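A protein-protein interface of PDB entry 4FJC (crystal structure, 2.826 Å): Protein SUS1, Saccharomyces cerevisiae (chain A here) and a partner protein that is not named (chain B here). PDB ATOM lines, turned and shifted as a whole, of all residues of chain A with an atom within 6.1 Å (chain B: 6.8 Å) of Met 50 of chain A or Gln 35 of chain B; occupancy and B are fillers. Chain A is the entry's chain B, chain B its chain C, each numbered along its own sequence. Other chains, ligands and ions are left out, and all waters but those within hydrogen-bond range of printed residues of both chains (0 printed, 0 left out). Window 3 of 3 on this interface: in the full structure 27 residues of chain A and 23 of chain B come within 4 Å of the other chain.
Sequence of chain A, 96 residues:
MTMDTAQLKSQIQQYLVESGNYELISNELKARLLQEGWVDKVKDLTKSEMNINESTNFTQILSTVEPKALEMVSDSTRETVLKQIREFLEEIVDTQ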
ATOM      1  N   LEU A  45      11.525  12.504 -27.929  1.00  0.00           N
ATOM      2  CA  LEU A  45      11.663  13.477 -26.857  1.00  0.00           C
ATOM      3  C   LEU A  45      10.337  14.114 -26.548  1.00  0.00           C
ATOM      4  O   LEU A  45      10.058  14.405 -25.394  1.00  0.00           O
ATOM      5  CB  LEU A  45      12.675  14.567 -27.230  1.00  0.00           C
ATOM      6  CG  LEU A  45      12.824  15.770 -26.275  1.00  0.00           C
ATOM      7  CD1 LEU A  45      13.202  15.344 -24.871  1.00  0.00           C
ATOM      8  CD2 LEU A  45      13.839  16.779 -26.814  1.00  0.00           C
ATOM      9  N   THR A  46       9.527  14.371 -27.567  1.00  0.00           N
ATOM     10  CA  THR A  46       8.225  14.982 -27.327  1.00  0.00           C
ATOM     11  C   THR A  46       7.377  14.011 -26.544  1.00  0.00           C
ATOM     12  O   THR A  46       6.726  14.397 -25.603  1.00  0.00           O
ATOM     13  CB  THR A  46       7.488  15.355 -28.614  1.00  0.00           C
ATOM     14  OG1 THR A  46       8.134  16.468 -29.231  1.00  0.00           O
ATOM     15  CG2 THR A  46       6.085  15.775 -28.295  1.00  0.00           C
ATOM     16  N   LYS A  47       7.399  12.744 -26.919  1.00  0.00           N
ATOM     17  CA  LYS A  47       6.676  11.725 -26.163  1.00  0.00           C
ATOM     18  C   LYS A  47       7.217  11.632 -24.745  1.00  0.00           C
ATOM     19  O   LYS A  47       6.475  11.532 -23.768  1.00  0.00           O
ATOM     20  CB  LYS A  47       6.750  10.363 -26.867  1.00  0.00           C
ATOM     21  CG  LYS A  47       6.120  10.400 -28.253  1.00  0.00           C
ATOM     22  CD  LYS A  47       5.463   9.083 -28.654  1.00  0.00           C
ATOM     23  CE  LYS A  47       5.846   8.680 -30.079  1.00  0.00           C
ATOM     24  NZ  LYS A  47       7.341   8.520 -30.176  1.00  0.00           N
ATOM     25  N   SER A  48       8.526  11.675 -24.632  1.00  0.00           N
ATOM     26  CA  SER A  48       9.129  11.600 -23.336  1.00  0.00           C
ATOM     27  C   SER A  48       8.632  12.745 -22.467  1.00  0.00           C
ATOM     28  O   SER A  48       8.332  12.558 -21.304  1.00  0.00           O
ATOM     29  CB  SER A  48      10.641  11.601 -23.462  1.00  0.00           C
ATOM     30  OG  SER A  48      11.238  11.823 -22.208  1.00  0.00           O
ATOM     31  N   GLU A  49       8.505  13.929 -23.031  1.00  0.00           N
ATOM     32  CA  GLU A  49       8.090  15.060 -22.231  1.00  0.00           C
ATOM     33  C   GLU A  49       6.619  14.984 -21.884  1.00  0.00           C
ATOM     34  O   GLU A  49       6.242  15.375 -20.783  1.00  0.00           O
ATOM     35  CB  GLU A  49       8.419  16.365 -22.933  1.00  0.00           C
ATOM     36  CG  GLU A  49       9.923  16.630 -23.046  1.00  0.00           C
ATOM     37  CD  GLU A  49      10.550  17.109 -21.744  1.00  0.00           C
ATOM     38  OE1 GLU A  49       9.833  17.190 -20.721  1.00  0.00           O
ATOM     39  OE2 GLU A  49      11.761  17.421 -21.736  1.00  0.00           O
ATOM     40  N   MET A  50       5.790  14.460 -22.786  1.00  0.00           N
ATOM     41  CA  MET A  50       4.355  14.323 -22.516  1.00  0.00           C
ATOM     42  C   MET A  50       4.140  13.428 -21.319  1.00  0.00           C
ATOM     43  O   MET A  50       3.200  13.599 -20.536  1.00  0.00           O
ATOM     44  CB  MET A  50       3.609  13.754 -23.723  1.00  0.00           C
ATOM     45  CG  MET A  50       3.232  14.831 -24.738  1.00  0.00           C
ATOM     46  SD  MET A  50       2.300  14.324 -26.212  1.00  0.00           S
ATOM     47  CE  MET A  50       3.355  13.031 -26.865  1.00  0.00           C
ATOM     48  N   ASN A  51       5.057  12.488 -21.176  1.00  0.00           N
ATOM     49  CA  ASN A  51       5.027  11.476 -20.143  1.00  0.00           C
ATOM     50  C   ASN A  51       5.461  12.065 -18.820  1.00  0.00           C
ATOM     51  O   ASN A  51       4.753  12.006 -17.835  1.00  0.00           O
ATOM     52  CB  ASN A  51       5.993  10.375 -20.558  1.00  0.00           C
ATOM     53  CG  ASN A  51       5.410   9.009 -20.405  1.00  0.00           C
ATOM     54  OD1 ASN A  51       5.330   8.493 -19.285  1.00  0.00           O
ATOM     55  ND2 ASN A  51       5.028   8.382 -21.537  1.00  0.00           N
ATOM     56  N   ILE A  52       6.640  12.658 -18.830  1.00  0.00           N
ATOM     57  CA  ILE A  52       7.237  13.234 -17.639  1.00  0.00           C
ATOM     58  C   ILE A  52       6.340  14.301 -17.032  1.00  0.00           C
ATOM     59  O   ILE A  52       6.254  14.397 -15.825  1.00  0.00           O
ATOM     60  CB  ILE A  52       8.596  13.863 -17.982  1.00  0.00           C
ATOM     61  CG1 ILE A  52       9.601  12.773 -18.303  1.00  0.00           C
ATOM     62  CG2 ILE A  52       9.109  14.744 -16.854  1.00  0.00           C
ATOM     63  CD1 ILE A  52      10.903  13.334 -18.801  1.00  0.00           C
ATOM     64  N   ASN A  53       5.680  15.093 -17.880  1.00  0.00           N
ATOM     65  CA  ASN A  53       4.818  16.196 -17.433  1.00  0.00           C
ATOM     66  C   ASN A  53       3.317  15.879 -17.377  1.00  0.00           C
ATOM     67  O   ASN A  53       2.494  16.757 -17.126  1.00  0.00           O
ATOM     68  CB  ASN A  53       5.055  17.379 -18.337  1.00  0.00           C
ATOM     69  CG  ASN A  53       6.435  17.934 -18.171  1.00  0.00           C
ATOM     70  OD1 ASN A  53       6.705  18.617 -17.193  1.00  0.00           O
ATOM     71  ND2 ASN A  53       7.324  17.632 -19.104  1.00  0.00           N
ATOM     72  N   GLU A  54       2.979  14.612 -17.594  1.00  0.00           N
ATOM     73  CA  GLU A  54       1.595  14.164 -17.648  1.00  0.00           C
ATOM     74  C   GLU A  54       0.707  15.210 -18.310  1.00  0.00           C
ATOM     75  O   GLU A  54      -0.275  15.663 -17.715  1.00  0.00           O
ATOM     76  CB  GLU A  54       1.078  13.804 -16.236  1.00  0.00           C
ATOM     77  CG  GLU A  54       1.807  12.649 -15.540  1.00  0.00           C
ATOM     78  CD  GLU A  54       1.767  11.304 -16.302  1.00  0.00           C
ATOM     79  OE1 GLU A  54       1.308  11.213 -17.473  1.00  0.00           O
ATOM     80  OE2 GLU A  54       2.229  10.296 -15.722  1.00  0.00           O
ATOM     81  N   SER A  55       1.067  15.572 -19.545  1.00  0.00           N
ATOM     82  CA  SER A  55       0.368  16.625 -20.295  1.00  0.00           C
ATOM     83  C   SER A  55       0.474  16.493 -21.827  1.00  0.00           C
ATOM     84  O   SER A  55       1.490  16.027 -22.345  1.00  0.00           O
ATOM     85  CB  SER A  55       0.891  18.019 -19.891  1.00  0.00           C
ATOM     86  OG  SER A  55       0.155  19.048 -20.553  1.00  0.00           O
ATOM     87  N   THR A  56      -0.581  16.928 -22.532  1.00  0.00           N
ATOM     88  CA  THR A  56      -0.565  16.978 -23.986  1.00  0.00           C
ATOM     89  C   THR A  56      -0.719  18.420 -24.479  1.00  0.00           C
ATOM     90  O   THR A  56      -1.063  18.649 -25.640  1.00  0.00           O
ATOM     91  CB  THR A  56      -1.690  16.140 -24.603  1.00  0.00           C
ATOM     92  OG1 THR A  56      -2.886  16.927 -24.627  1.00  0.00           O
ATOM     93  CG2 THR A  56      -1.933  14.877 -23.833  1.00  0.00           C
ATOM     94  N   ASN A  57      -0.475  19.384 -23.586  1.00  0.00           N
ATOM     95  CA  ASN A  57      -0.635  20.817 -23.893  1.00  0.00           C
ATOM     96  C   ASN A  57       0.532  21.280 -24.724  1.00  0.00           C
ATOM     97  O   ASN A  57       1.681  21.154 -24.322  1.00  0.00           O
ATOM     98  CB  ASN A  57      -0.688  21.647 -22.610  1.00  0.00           C
ATOM     99  CG  ASN A  57      -0.915  23.126 -22.870  1.00  0.00           C
ATOM    100  OD1 ASN A  57       0.014  23.898 -23.240  1.00  0.00           O
ATOM    101  ND2 ASN A  57      -2.163  23.541 -22.663  1.00  0.00           N
ATOM    102  N   ILE A  61       4.407  21.848 -23.507  1.00  0.00           N
ATOM    103  CA  ILE A  61       5.319  20.813 -24.082  1.00  0.00           C
ATOM    104  C   ILE A  61       6.354  21.370 -25.065  1.00  0.00           C
ATOM    105  O   ILE A  61       7.485  20.961 -25.033  1.00  0.00           O
ATOM    106  CB  ILE A  61       4.556  19.666 -24.797  1.00  0.00           C
ATOM    107  CG1 ILE A  61       3.853  18.762 -23.795  1.00  0.00           C
ATOM    108  CG2 ILE A  61       5.502  18.789 -25.573  1.00  0.00           C
ATOM    109  CD1 ILE A  61       4.771  18.160 -22.740  1.00  0.00           C
ATOM    110  N   VAL B  28       6.074  18.601 -32.931  1.00  0.00           N
ATOM    111  CA  VAL B  28       5.448  18.644 -31.611  1.00  0.00           C
ATOM    112  C   VAL B  28       3.936  18.791 -31.745  1.00  0.00           C
ATOM    113  O   VAL B  28       3.199  18.075 -31.077  1.00  0.00           O
ATOM    114  CB  VAL B  28       6.033  19.781 -30.714  1.00  0.00           C
ATOM    115  CG1 VAL B  28       5.167  19.990 -29.480  1.00  0.00           C
ATOM    116  CG2 VAL B  28       7.463  19.465 -30.291  1.00  0.00           C
ATOM    117  N   ARG B  30       2.229  17.650 -34.031  1.00  0.00           N
ATOM    118  CA  ARG B  30       1.661  16.423 -34.532  1.00  0.00           C
ATOM    119  C   ARG B  30       1.631  15.359 -33.501  1.00  0.00           C
ATOM    120  O   ARG B  30       0.867  14.420 -33.631  1.00  0.00           O
ATOM    121  CB  ARG B  30       2.439  15.906 -35.708  1.00  0.00           C
ATOM    122  CG  ARG B  30       2.137  16.593 -37.015  1.00  0.00           C
ATOM    123  CD  ARG B  30       3.284  16.267 -37.942  1.00  0.00           C
ATOM    124  NE  ARG B  30       3.286  17.127 -39.092  1.00  0.00           N
ATOM    125  CZ  ARG B  30       2.647  16.853 -40.205  1.00  0.00           C
ATOM    126  NH1 ARG B  30       1.943  15.746 -40.321  1.00  0.00           N
ATOM    127  NH2 ARG B  30       2.727  17.702 -41.208  1.00  0.00           N
ATOM    128  N   GLU B  31       2.490  15.477 -32.504  1.00  0.00           N
ATOM    129  CA  GLU B  31       2.607  14.463 -31.467  1.00  0.00           C
ATOM    130  C   GLU B  31       1.639  14.749 -30.355  1.00  0.00           C
ATOM    131  O   GLU B  31       1.086  13.812 -29.771  1.00  0.00           O
ATOM    132  CB  GLU B  31       4.009  14.436 -30.877  1.00  0.00           C
ATOM    133  CG  GLU B  31       5.083  13.883 -31.793  1.00  0.00           C
ATOM    134  CD  GLU B  31       5.018  12.379 -31.975  1.00  0.00           C
ATOM    135  OE1 GLU B  31       4.368  11.639 -31.160  1.00  0.00           O
ATOM    136  OE2 GLU B  31       5.674  11.932 -32.950  1.00  0.00           O
ATOM    137  N   THR B  32       1.450  16.036 -30.053  1.00  0.00           N
ATOM    138  CA  THR B  32       0.625  16.437 -28.903  1.00  0.00           C
ATOM    139  C   THR B  32      -0.834  16.151 -29.188  1.00  0.00           C
ATOM    140  O   THR B  32      -1.563  15.664 -28.319  1.00  0.00           O
ATOM    141  CB  THR B  32       0.792  17.932 -28.507  1.00  0.00           C
ATOM    142  OG1 THR B  32       0.419  18.785 -29.599  1.00  0.00           O
ATOM    143  CG2 THR B  32       2.226  18.242 -28.090  1.00  0.00           C
ATOM    144  N   THR B  33      -1.244  16.452 -30.416  1.00  0.00           N
ATOM    145  CA  THR B  33      -2.623  16.265 -30.855  1.00  0.00           C
ATOM    146  C   THR B  33      -2.936  14.788 -30.940  1.00  0.00           C
ATOM    147  O   THR B  33      -3.932  14.303 -30.432  1.00  0.00           O
ATOM    148  CB  THR B  33      -2.818  16.873 -32.244  1.00  0.00           C
ATOM    149  OG1 THR B  33      -1.779  16.403 -33.107  1.00  0.00           O
ATOM    150  CG2 THR B  33      -2.740  18.391 -32.189  1.00  0.00           C
ATOM    151  N   GLN B  34      -2.053  14.069 -31.595  1.00  0.00           N
ATOM    152  CA  GLN B  34      -2.258  12.677 -31.865  1.00  0.00           C
ATOM    153  C   GLN B  34      -2.442  11.957 -30.527  1.00  0.00           C
ATOM    154  O   GLN B  34      -3.178  10.973 -30.439  1.00  0.00           O
ATOM    155  CB  GLN B  34      -1.032  12.186 -32.633  1.00  0.00           C
ATOM    156  CG  GLN B  34      -1.064  10.797 -33.230  1.00  0.00           C
ATOM    157  CD  GLN B  34       0.340  10.265 -33.501  1.00  0.00           C
ATOM    158  OE1 GLN B  34       1.174  10.962 -34.094  1.00  0.00           O
ATOM    159  NE2 GLN B  34       0.614   9.036 -33.055  1.00  0.00           N
ATOM    160  N   GLN B  35      -1.768  12.454 -29.488  1.00  0.00           N
ATOM    161  CA  GLN B  35      -1.755  11.823 -28.169  1.00  0.00           C
ATOM    162  C   GLN B  35      -2.961  12.287 -27.345  1.00  0.00           C
ATOM    163  O   GLN B  35      -3.528  11.517 -26.587  1.00  0.00           O
ATOM    164  CB  GLN B  35      -0.432  12.176 -27.467  1.00  0.00           C
ATOM    165  CG  GLN B  35      -0.230  11.620 -26.074  1.00  0.00           C
ATOM    166  CD  GLN B  35      -0.275  10.105 -26.023  1.00  0.00           C
ATOM    167  OE1 GLN B  35      -0.198   9.417 -27.050  1.00  0.00           O
ATOM    168  NE2 GLN B  35      -0.388   9.574 -24.818  1.00  0.00           N
ATOM    169  N   GLN B  36      -3.344  13.549 -27.492  1.00  0.00           N
ATOM    170  CA  GLN B  36      -4.596  14.037 -26.940  1.00  0.00           C
ATOM    171  C   GLN B  36      -5.743  13.138 -27.418  1.00  0.00           C
ATOM    172  O   GLN B  36      -6.529  12.660 -26.618  1.00  0.00           O
ATOM    173  CB  GLN B  36      -4.832  15.512 -27.345  1.00  0.00           C
ATOM    174  CG  GLN B  36      -6.027  16.164 -26.686  1.00  0.00           C
ATOM    175  CD  GLN B  36      -6.396  17.526 -27.276  1.00  0.00           C
ATOM    176  OE1 GLN B  36      -6.645  17.648 -28.463  1.00  0.00           O
ATOM    177  NE2 GLN B  36      -6.498  18.539 -26.431  1.00  0.00           N
ATOM    178  N   LEU B  37      -5.819  12.913 -28.727  1.00  0.00           N
ATOM    179  CA  LEU B  37      -6.843  12.074 -29.323  1.00  0.00           C
ATOM    180  C   LEU B  37      -6.874  10.697 -28.688  1.00  0.00           C
ATOM    181  O   LEU B  37      -7.942  10.240 -28.346  1.00  0.00           O
ATOM    182  CB  LEU B  37      -6.622  11.909 -30.830  1.00  0.00           C
ATOM    183  CG  LEU B  37      -7.619  10.962 -31.529  1.00  0.00           C
ATOM    184  CD1 LEU B  37      -9.005  11.559 -31.360  1.00  0.00           C
ATOM    185  CD2 LEU B  37      -7.345  10.699 -33.004  1.00  0.00           C
ATOM    186  N   LEU B  38      -5.728  10.031 -28.547  1.00  0.00           N
ATOM    187  CA  LEU B  38      -5.701   8.684 -27.967  1.00  0.00           C
ATOM    188  C   LEU B  38      -6.147   8.619 -26.502  1.00  0.00           C
ATOM    189  O   LEU B  38      -6.734   7.632 -26.102  1.00  0.00           O
ATOM    190  CB  LEU B  38      -4.325   8.012 -28.141  1.00  0.00           C
ATOM    191  CG  LEU B  38      -4.182   7.361 -29.533  1.00  0.00           C
ATOM    192  CD1 LEU B  38      -2.823   7.610 -30.222  1.00  0.00           C
ATOM    193  CD2 LEU B  38      -4.538   5.878 -29.488  1.00  0.00           C
ATOM    194  N   LYS B  39      -5.892   9.669 -25.727  1.00  0.00           N
ATOM    195  CA  LYS B  39      -6.283   9.723 -24.318  1.00  0.00           C
ATOM    196  C   LYS B  39      -7.777  10.018 -24.113  1.00  0.00           C
ATOM    197  O   LYS B  39      -8.407   9.475 -23.215  1.00  0.00           O
ATOM    198  CB  LYS B  39      -5.413  10.745 -23.554  1.00  0.00           C
ATOM    199  CG  LYS B  39      -4.029  10.197 -23.170  1.00  0.00           C
ATOM    200  CD  LYS B  39      -3.116  11.187 -22.431  1.00  0.00           C
ATOM    201  CE  LYS B  39      -3.043  10.934 -20.924  1.00  0.00           C
ATOM    202  NZ  LYS B  39      -2.997   9.478 -20.499  1.00  0.00           N
ATOM    203  N   THR B  40      -8.330  10.891 -24.936  1.00  0.00           N
ATOM    204  CA  THR B  40      -9.773  11.145 -24.978  1.00  0.00           C
ATOM    205  C   THR B  40     -10.545   9.929 -25.509  1.00  0.00           C
ATOM    206  O   THR B  40     -11.657   9.653 -25.098  1.00  0.00           O
ATOM    207  CB  THR B  40     -10.063  12.330 -25.918  1.00  0.00           C
ATOM    208  OG1 THR B  40      -8.970  13.253 -25.865  1.00  0.00           O
ATOM    209  CG2 THR B  40     -11.334  13.044 -25.549  1.00  0.00           C
ATOM    210  N   LEU B  45      -5.681   2.462 -20.848  1.00  0.00           N
ATOM    211  CA  LEU B  45      -4.547   2.367 -21.756  1.00  0.00           C
ATOM    212  C   LEU B  45      -3.465   1.460 -21.181  1.00  0.00           C
ATOM    213  O   LEU B  45      -2.323   1.491 -21.629  1.00  0.00           O
ATOM    214  CB  LEU B  45      -3.991   3.767 -22.019  1.00  0.00           C
ATOM    215  CG  LEU B  45      -3.609   4.573 -20.762  1.00  0.00           C
ATOM    216  CD1 LEU B  45      -2.126   4.411 -20.400  1.00  0.00           C
ATOM    217  CD2 LEU B  45      -4.002   6.042 -20.940  1.00  0.00           C
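O of Glu 31 of chain B sits close to SD of Met 50 of chain A (3.8 Å).
The backbone NH of Ser 55 of chain A is in hydrogen-bond range of the backbone carbonyl oxygen of Met 50 of chain A, at 3.1 Å.
The backbone carbonyl oxygen (O) of Val 28 of chain B lies close to the side-chain hydroxyl (OG1) of Thr 32 of chain B, 3.2 Å away.
The backbone carbonyl oxygen (O) of Gln 36 of chain B is in hydrogen-bond range of the side-chain hydroxyl (OG1) of Thr 40 of chain B (2.6 Å).
Among the printed residues, merely in contact across the chains: Thr 46 of chain A with Val 28 of chain B, Thr 46 of chain A with Glu 31 of chain B, Lys 47 of chain A with Glu 31 of chain B, Met 50 of chain A with Thr 32 of chain B, Met 50 of chain A with Gln 35 of chain B, Thr 56 of chain A with Thr 32 of chain B and Thr 56 of chain A with Gln 36 of chain B.
Met 50 of chain A touches just these residues of chain B: Glu 31 (3.8 Å), Thr 32 (3.8 Å) and Gln 35 (3.7 Å).
Gln 35 of chain B touches just one residue of chain A: Met 50.
Of the printed residues of chain B, Thr 46 of chain A touches Val 28 (3.2 Å) and Glu 31 (3.6 Å).
Printed residues of chain B within 4 Å of Thr 56 of chain A: Thr 32 and Gln 36.
Of the printed residues of chain A, Gln 36 of chain B touches Thr 56 (3.6 Å).
Of the printed residues of chain A, Val 28 of chain B touches Thr 46 (3.2 Å).
Lys 39 of chain B touches none of the printed residues of chain A.
Leu 45 of chain A touches none of the printed residues of chain B.
The nearest residue of chain B that does not touch Met 50 of chain A is Gln 36 of chain B (5.8 Å).
The nearest printed residue of chain A that does not touch Thr 32 of chain B is Ile 61 of chain A (4.2 Å).
Printed residues of chain A that touch a printed residue of chain B: Thr 46, Lys 47, Met 50 and Thr 56.
Hydrophobic or aromatic side chains of chain A within 4 Å of the printed part of chain B: Met 50.
Of the 13 printed residues of chain B, 5 touch a printed residue of chain A.
Printed residues of chain B that touch a printed residue of chain A: Val 28, Glu 31, Thr 32, Gln 35 and Gln 36.
Among the printed residues, 8 pairs touch across the chains.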
